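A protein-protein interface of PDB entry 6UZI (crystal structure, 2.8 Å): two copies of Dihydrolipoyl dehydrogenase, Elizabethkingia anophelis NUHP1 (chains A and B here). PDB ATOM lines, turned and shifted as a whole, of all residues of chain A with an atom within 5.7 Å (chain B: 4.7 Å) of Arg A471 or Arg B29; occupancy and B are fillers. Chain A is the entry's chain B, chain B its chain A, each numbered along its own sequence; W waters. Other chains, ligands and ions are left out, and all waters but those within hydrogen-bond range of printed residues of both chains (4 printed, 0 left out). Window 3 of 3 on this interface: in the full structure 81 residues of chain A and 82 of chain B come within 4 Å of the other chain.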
ATOM      1  N   GLU A 444     -24.520 -11.034 -30.040  1.00  0.00           N
ATOM      2  CA  GLU A 444     -24.701 -11.125 -28.595  1.00  0.00           C
ATOM      3  C   GLU A 444     -26.137 -11.490 -28.239  1.00  0.00           C
ATOM      4  O   GLU A 444     -26.365 -12.326 -27.353  1.00  0.00           O
ATOM      5  CB  GLU A 444     -24.301  -9.805 -27.932  1.00  0.00           C
ATOM      6  CG  GLU A 444     -24.473  -9.766 -26.409  1.00  0.00           C
ATOM      7  CD  GLU A 444     -23.959  -8.475 -25.784  1.00  0.00           C
ATOM      8  OE1 GLU A 444     -23.513  -7.583 -26.537  1.00  0.00           O
ATOM      9  OE2 GLU A 444     -24.007  -8.344 -24.541  1.00  0.00           O
ATOM     10  N   ALA A 447     -26.682 -15.118 -28.581  1.00  0.00           N
ATOM     11  CA  ALA A 447     -25.852 -15.812 -27.604  1.00  0.00           C
ATOM     12  C   ALA A 447     -26.451 -15.774 -26.202  1.00  0.00           C
ATOM     13  O   ALA A 447     -26.072 -16.586 -25.355  1.00  0.00           O
ATOM     14  CB  ALA A 447     -24.448 -15.212 -27.600  1.00  0.00           C
ATOM     15  N   ARG A 448     -27.360 -14.844 -25.931  1.00  0.00           N
ATOM     16  CA  ARG A 448     -27.938 -14.706 -24.607  1.00  0.00           C
ATOM     17  C   ARG A 448     -29.318 -15.337 -24.494  1.00  0.00           C
ATOM     18  O   ARG A 448     -29.857 -15.418 -23.384  1.00  0.00           O
ATOM     19  CB  ARG A 448     -28.012 -13.220 -24.215  1.00  0.00           C
ATOM     20  CG  ARG A 448     -26.649 -12.622 -23.902  1.00  0.00           C
ATOM     21  CD  ARG A 448     -26.690 -11.149 -23.476  1.00  0.00           C
ATOM     22  NE  ARG A 448     -25.338 -10.659 -23.197  1.00  0.00           N
ATOM     23  CZ  ARG A 448     -24.641 -10.965 -22.100  1.00  0.00           C
ATOM     24  NH1 ARG A 448     -25.166 -11.762 -21.177  1.00  0.00           N
ATOM     25  NH2 ARG A 448     -23.416 -10.481 -21.924  1.00  0.00           N
ATOM     26  N   LEU A 465     -21.910 -16.927 -29.767  1.00  0.00           N
ATOM     27  CA  LEU A 465     -20.921 -16.595 -28.745  1.00  0.00           C
ATOM     28  C   LEU A 465     -19.528 -16.444 -29.347  1.00  0.00           C
ATOM     29  O   LEU A 465     -18.751 -15.582 -28.922  1.00  0.00           O
ATOM     30  CB  LEU A 465     -20.914 -17.664 -27.655  1.00  0.00           C
ATOM     31  CG  LEU A 465     -21.991 -17.664 -26.570  1.00  0.00           C
ATOM     32  CD1 LEU A 465     -21.917 -18.976 -25.835  1.00  0.00           C
ATOM     33  CD2 LEU A 465     -21.810 -16.507 -25.602  1.00  0.00           C
ATOM     34  N   ASP A 466     -19.180 -17.295 -30.313  1.00  0.00           N
ATOM     35  CA  ASP A 466     -17.871 -17.184 -30.952  1.00  0.00           C
ATOM     36  C   ASP A 466     -17.764 -15.909 -31.769  1.00  0.00           C
ATOM     37  O   ASP A 466     -16.711 -15.261 -31.787  1.00  0.00           O
ATOM     38  CB  ASP A 466     -17.596 -18.404 -31.830  1.00  0.00           C
ATOM     39  CG  ASP A 466     -16.178 -18.430 -32.364  1.00  0.00           C
ATOM     40  OD1 ASP A 466     -15.232 -18.316 -31.556  1.00  0.00           O
ATOM     41  OD2 ASP A 466     -16.008 -18.584 -33.594  1.00  0.00           O
ATOM     42  N   THR A 468     -19.553 -13.019 -31.383  1.00  0.00           N
ATOM     43  CA  THR A 468     -19.703 -11.766 -30.654  1.00  0.00           C
ATOM     44  C   THR A 468     -18.432 -11.402 -29.899  1.00  0.00           C
ATOM     45  O   THR A 468     -18.087 -10.218 -29.802  1.00  0.00           O
ATOM     46  CB  THR A 468     -20.896 -11.840 -29.702  1.00  0.00           C
ATOM     47  OG1 THR A 468     -21.217 -10.525 -29.239  1.00  0.00           O
ATOM     48  CG2 THR A 468     -20.604 -12.748 -28.491  1.00  0.00           C
ATOM     49  N   GLY A 469     -17.712 -12.396 -29.374  1.00  0.00           N
ATOM     50  CA  GLY A 469     -16.543 -12.112 -28.562  1.00  0.00           C
ATOM     51  C   GLY A 469     -15.591 -13.271 -28.354  1.00  0.00           C
ATOM     52  O   GLY A 469     -14.896 -13.316 -27.334  1.00  0.00           O
ATOM     53  N   LYS A 470     -15.557 -14.211 -29.305  1.00  0.00           N
ATOM     54  CA  LYS A 470     -14.678 -15.383 -29.239  1.00  0.00           C
ATOM     55  C   LYS A 470     -14.804 -16.092 -27.891  1.00  0.00           C
ATOM     56  O   LYS A 470     -13.819 -16.566 -27.321  1.00  0.00           O
ATOM     57  CB  LYS A 470     -13.219 -14.991 -29.502  1.00  0.00           C
ATOM     58  CG  LYS A 470     -12.930 -14.378 -30.856  1.00  0.00           C
ATOM     59  CD  LYS A 470     -12.504 -15.422 -31.875  1.00  0.00           C
ATOM     60  CE  LYS A 470     -12.582 -14.895 -33.310  1.00  0.00           C
ATOM     61  NZ  LYS A 470     -13.996 -14.741 -33.783  1.00  0.00           N
ATOM     62  N   ARG A 471     -16.032 -16.189 -27.385  1.00  0.00           N
ATOM     63  CA  ARG A 471     -16.254 -16.701 -26.036  1.00  0.00           C
ATOM     64  C   ARG A 471     -17.332 -17.782 -26.033  1.00  0.00           C
ATOM     65  O   ARG A 471     -18.256 -17.780 -25.217  1.00  0.00           O
ATOM     66  CB  ARG A 471     -16.601 -15.580 -25.051  1.00  0.00           C
ATOM     67  CG  ARG A 471     -17.747 -14.646 -25.440  1.00  0.00           C
ATOM     68  CD  ARG A 471     -18.086 -13.726 -24.273  1.00  0.00           C
ATOM     69  NE  ARG A 471     -19.269 -12.909 -24.516  1.00  0.00           N
ATOM     70  CZ  ARG A 471     -20.482 -13.165 -24.019  1.00  0.00           C
ATOM     71  NH1 ARG A 471     -20.690 -14.223 -23.242  1.00  0.00           N
ATOM     72  NH2 ARG A 471     -21.499 -12.358 -24.297  1.00  0.00           N
ATOM     73  N   ALA A 472     -17.231 -18.722 -26.966  1.00  0.00           N
ATOM     74  CA  ALA A 472     -18.070 -19.906 -26.910  1.00  0.00           C
ATOM     75  C   ALA A 472     -17.728 -20.729 -25.670  1.00  0.00           C
ATOM     76  O   ALA A 472     -16.601 -20.700 -25.168  1.00  0.00           O
ATOM     77  CB  ALA A 472     -17.897 -20.751 -28.170  1.00  0.00           C
ATOM     78  N   ILE A 473     -18.724 -21.458 -25.175  1.00  0.00           N
ATOM     79  CA  ILE A 473     -18.600 -22.209 -23.928  1.00  0.00           C
ATOM     80  C   ILE A 473     -18.106 -23.633 -24.164  1.00  0.00           C
ATOM     81  O   ILE A 473     -17.258 -24.129 -23.417  1.00  0.00           O
ATOM     82  CB  ILE A 473     -19.953 -22.200 -23.189  1.00  0.00           C
ATOM     83  CG1 ILE A 473     -20.313 -20.775 -22.761  1.00  0.00           C
ATOM     84  CG2 ILE A 473     -19.929 -23.152 -21.997  1.00  0.00           C
ATOM     85  CD1 ILE A 473     -19.455 -20.254 -21.617  1.00  0.00           C
ATOM     86  N   VAL B  25     -20.678 -25.105 -16.954  1.00  0.00           N
ATOM     87  CA  VAL B  25     -20.806 -23.903 -17.770  1.00  0.00           C
ATOM     88  C   VAL B  25     -20.515 -22.666 -16.930  1.00  0.00           C
ATOM     89  O   VAL B  25     -19.793 -21.764 -17.363  1.00  0.00           O
ATOM     90  CB  VAL B  25     -22.196 -23.842 -18.427  1.00  0.00           C
ATOM     91  CG1 VAL B  25     -22.476 -22.456 -18.974  1.00  0.00           C
ATOM     92  CG2 VAL B  25     -22.282 -24.878 -19.545  1.00  0.00           C
ATOM     93  N   ALA B  26     -21.013 -22.635 -15.694  1.00  0.00           N
ATOM     94  CA  ALA B  26     -20.686 -21.533 -14.794  1.00  0.00           C
ATOM     95  C   ALA B  26     -19.183 -21.411 -14.589  1.00  0.00           C
ATOM     96  O   ALA B  26     -18.642 -20.300 -14.569  1.00  0.00           O
ATOM     97  CB  ALA B  26     -21.389 -21.720 -13.452  1.00  0.00           C
ATOM     98  N   ALA B  27     -18.495 -22.543 -14.413  1.00  0.00           N
ATOM     99  CA  ALA B  27     -17.049 -22.502 -14.220  1.00  0.00           C
ATOM    100  C   ALA B  27     -16.344 -21.915 -15.435  1.00  0.00           C
ATOM    101  O   ALA B  27     -15.463 -21.060 -15.294  1.00  0.00           O
ATOM    102  CB  ALA B  27     -16.516 -23.903 -13.914  1.00  0.00           C
ATOM    103  N   ILE B  28     -16.739 -22.335 -16.639  1.00  0.00           N
ATOM    104  CA  ILE B  28     -16.111 -21.808 -17.849  1.00  0.00           C
ATOM    105  C   ILE B  28     -16.326 -20.307 -17.943  1.00  0.00           C
ATOM    106  O   ILE B  28     -15.403 -19.547 -18.262  1.00  0.00           O
ATOM    107  CB  ILE B  28     -16.655 -22.530 -19.095  1.00  0.00           C
ATOM    108  CG1 ILE B  28     -16.234 -23.999 -19.088  1.00  0.00           C
ATOM    109  CG2 ILE B  28     -16.188 -21.845 -20.361  1.00  0.00           C
ATOM    110  CD1 ILE B  28     -16.839 -24.802 -20.208  1.00  0.00           C
ATOM    111  N   ARG B  29     -17.545 -19.854 -17.656  1.00  0.00           N
ATOM    112  CA  ARG B  29     -17.818 -18.427 -17.718  1.00  0.00           C
ATOM    113  C   ARG B  29     -17.044 -17.664 -16.648  1.00  0.00           C
ATOM    114  O   ARG B  29     -16.610 -16.532 -16.890  1.00  0.00           O
ATOM    115  CB  ARG B  29     -19.323 -18.187 -17.596  1.00  0.00           C
ATOM    116  CG  ARG B  29     -19.765 -16.786 -17.962  1.00  0.00           C
ATOM    117  CD  ARG B  29     -19.749 -16.601 -19.453  1.00  0.00           C
ATOM    118  NE  ARG B  29     -20.008 -15.210 -19.802  1.00  0.00           N
ATOM    119  CZ  ARG B  29     -19.080 -14.360 -20.229  1.00  0.00           C
ATOM    120  NH1 ARG B  29     -17.827 -14.767 -20.370  1.00  0.00           N
ATOM    121  NH2 ARG B  29     -19.409 -13.111 -20.520  1.00  0.00           N
ATOM    122  N   CYS B  30     -16.842 -18.267 -15.471  1.00  0.00           N
ATOM    123  CA  CYS B  30     -16.006 -17.633 -14.453  1.00  0.00           C
ATOM    124  C   CYS B  30     -14.556 -17.563 -14.904  1.00  0.00           C
ATOM    125  O   CYS B  30     -13.872 -16.558 -14.675  1.00  0.00           O
ATOM    126  CB  CYS B  30     -16.116 -18.381 -13.123  1.00  0.00           C
ATOM    127  SG  CYS B  30     -17.618 -18.008 -12.197  1.00  0.00           S
ATOM    128  N   ALA B  31     -14.065 -18.632 -15.529  1.00  0.00           N
ATOM    129  CA  ALA B  31     -12.712 -18.606 -16.065  1.00  0.00           C
ATOM    130  C   ALA B  31     -12.579 -17.586 -17.199  1.00  0.00           C
ATOM    131  O   ALA B  31     -11.547 -16.912 -17.312  1.00  0.00           O
ATOM    132  CB  ALA B  31     -12.316 -20.007 -16.530  1.00  0.00           C
ATOM    133  N   GLN B  32     -13.606 -17.456 -18.048  1.00  0.00           N
ATOM    134  CA  GLN B  32     -13.526 -16.489 -19.140  1.00  0.00           C
ATOM    135  C   GLN B  32     -13.485 -15.059 -18.618  1.00  0.00           C
ATOM    136  O   GLN B  32     -12.894 -14.182 -19.258  1.00  0.00           O
ATOM    137  CB  GLN B  32     -14.695 -16.667 -20.109  1.00  0.00           C
ATOM    138  CG  GLN B  32     -14.671 -17.968 -20.904  1.00  0.00           C
ATOM    139  CD  GLN B  32     -15.853 -18.097 -21.865  1.00  0.00           C
ATOM    140  OE1 GLN B  32     -16.842 -17.370 -21.757  1.00  0.00           O
ATOM    141  NE2 GLN B  32     -15.767 -19.057 -22.783  1.00  0.00           N
ATOM    142  N   LEU B  33     -14.095 -14.802 -17.465  1.00  0.00           N
ATOM    143  CA  LEU B  33     -14.131 -13.462 -16.897  1.00  0.00           C
ATOM    144  C   LEU B  33     -12.915 -13.156 -16.031  1.00  0.00           C
ATOM    145  O   LEU B  33     -12.791 -12.035 -15.533  1.00  0.00           O
ATOM    146  CB  LEU B  33     -15.424 -13.262 -16.101  1.00  0.00           C
ATOM    147  CG  LEU B  33     -16.684 -13.286 -16.980  1.00  0.00           C
ATOM    148  CD1 LEU B  33     -17.948 -13.476 -16.161  1.00  0.00           C
ATOM    149  CD2 LEU B  33     -16.791 -12.014 -17.806  1.00  0.00           C
ATOM    150  N   VAL B 337     -24.189 -18.889 -16.260  1.00  0.00           N
ATOM    151  CA  VAL B 337     -23.643 -17.711 -16.930  1.00  0.00           C
ATOM    152  C   VAL B 337     -24.089 -16.439 -16.222  1.00  0.00           C
ATOM    153  O   VAL B 337     -23.337 -15.461 -16.129  1.00  0.00           O
ATOM    154  CB  VAL B 337     -24.054 -17.696 -18.414  1.00  0.00           C
ATOM    155  CG1 VAL B 337     -23.565 -16.426 -19.079  1.00  0.00           C
ATOM    156  CG2 VAL B 337     -23.505 -18.917 -19.122  1.00  0.00           C
ATOM    157  N   ALA B 340     -21.897 -15.944 -12.997  1.00  0.00           N
ATOM    158  CA  ALA B 340     -20.528 -15.571 -13.340  1.00  0.00           C
ATOM    159  C   ALA B 340     -20.448 -14.112 -13.770  1.00  0.00           C
ATOM    160  O   ALA B 340     -19.572 -13.366 -13.316  1.00  0.00           O
ATOM    161  CB  ALA B 340     -19.992 -16.487 -14.443  1.00  0.00           C
ATOM    162  N   GLU B 341     -21.362 -13.680 -14.642  1.00  0.00           N
ATOM    163  CA  GLU B 341     -21.340 -12.290 -15.080  1.00  0.00           C
ATOM    164  C   GLU B 341     -21.710 -11.345 -13.945  1.00  0.00           C
ATOM    165  O   GLU B 341     -21.145 -10.250 -13.843  1.00  0.00           O
ATOM    166  CB  GLU B 341     -22.273 -12.119 -16.278  1.00  0.00           C
ATOM    167  CG  GLU B 341     -21.717 -12.747 -17.541  1.00  0.00           C
ATOM    168  CD  GLU B 341     -22.705 -12.778 -18.675  1.00  0.00           C
ATOM    169  OE1 GLU B 341     -23.759 -12.128 -18.556  1.00  0.00           O
ATOM    170  OE2 GLU B 341     -22.427 -13.458 -19.686  1.00  0.00           O
HETATM  171  O   HOH W   1     -19.308 -16.790 -23.263  1.00  0.00           O
HETATM  172  O   HOH W   2     -20.816 -10.321 -20.970  1.00  0.00           O
HETATM  173  O   HOH W   3     -24.117  -9.392 -18.790  1.00  0.00           O
HETATM  174  O   HOH W   4     -23.288 -13.992 -22.068  1.00  0.00           O
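Among the printed residues, merely in contact across the chains: Ile A473 with Ile B28, Arg A471 with Gln B32, Ile A473 with Val B25 and Ile A473 with Gln B32.
The backbone carbonyl oxygen of Ala A472 is in hydrogen-bond range of the side-chain amide nitrogen of Gln B32. The guanidinium group of Arg A448 lies within salt-bridge range of the side-chain carboxylate of Glu B341 (3.0 Å). The guanidinium group of Arg B29 sits close to the guanidinium group of Arg A471 (3.2 Å).
Of the printed residues of chain B, Arg A448 touches Glu B341. Leu A465 touches none of the printed residues of chain B. Of chain B, only Arg B29 (3.2 Å) and Gln B32 (3.7 Å) come within 4 Å of Arg A471. Printed residues of chain B within 4 Å of Ile A473: Val B25 (3.8 Å), Ile B28 (3.3 Å) and Gln B32 (3.9 Å). Of the printed residues of chain A, Val B25 touches Ile A473. Of the printed residues of chain A, Ile B28 touches Ile A473 (3.3 Å). Of chain A, only Arg A471 (3.2 Å) comes within 4 Å of Arg B29. The nearest residue of chain A that does not touch Arg B29 is Ile A473 (4.3 Å). The nearest printed residue of chain A that does not touch Val B25 is Leu A465 (7.7 Å).
NH1 of Arg B29 lies within hydrogen-bond range of OE1 of Gln B32, at 3.1 Å. The guanidinium group (NE) of Arg B29 is in salt-bridge range of the side-chain carboxylate (OE2) of Glu B341, 3.0 Å away. NE of Arg A448 lies within salt-bridge range of OE2 of Glu A444 (3.0 Å). The backbone NH (N) of Arg A471 sits at hydrogen-bond distance from the backbone carbonyl oxygen (O) of Leu A465.
Water W1 bridges O of Arg A471 and OE1 of Gln B32. Water W4 lies within hydrogen-bond range of OE2 of Glu B341 (2.6 Å), NH1 of Arg A471 (2.9 Å) and NH1 of Arg A448 (3.0 Å). Water W3 lies within hydrogen-bond range of OE1 of Glu B341 (2.8 Å) and NH2 of Arg A448 (3.4 Å). Water W2 bridges NH2 of Arg A448 (2.8 Å) and NH2 of Arg B29 (3.2 Å).
Printed residues of chain A that touch a printed residue of chain B: Arg A448, Arg A471, Ala A472 and Ile A473. Hydrophobic or aromatic side chains of chain B within 4 Å of the printed part of chain A: Val B25 and Ile B28. Along chain B the printed residues that touch a printed residue of chain A span positions 25 to 341. Among the printed residues, 7 pairs touch across the chains. Among the printed residues, Asp or Glu carboxylates within 4 Å of a Lys or Arg side-chain nitrogen of the other chain: Arg A448 with Glu B341 (3.0 Å).
No position is printed for both chains.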
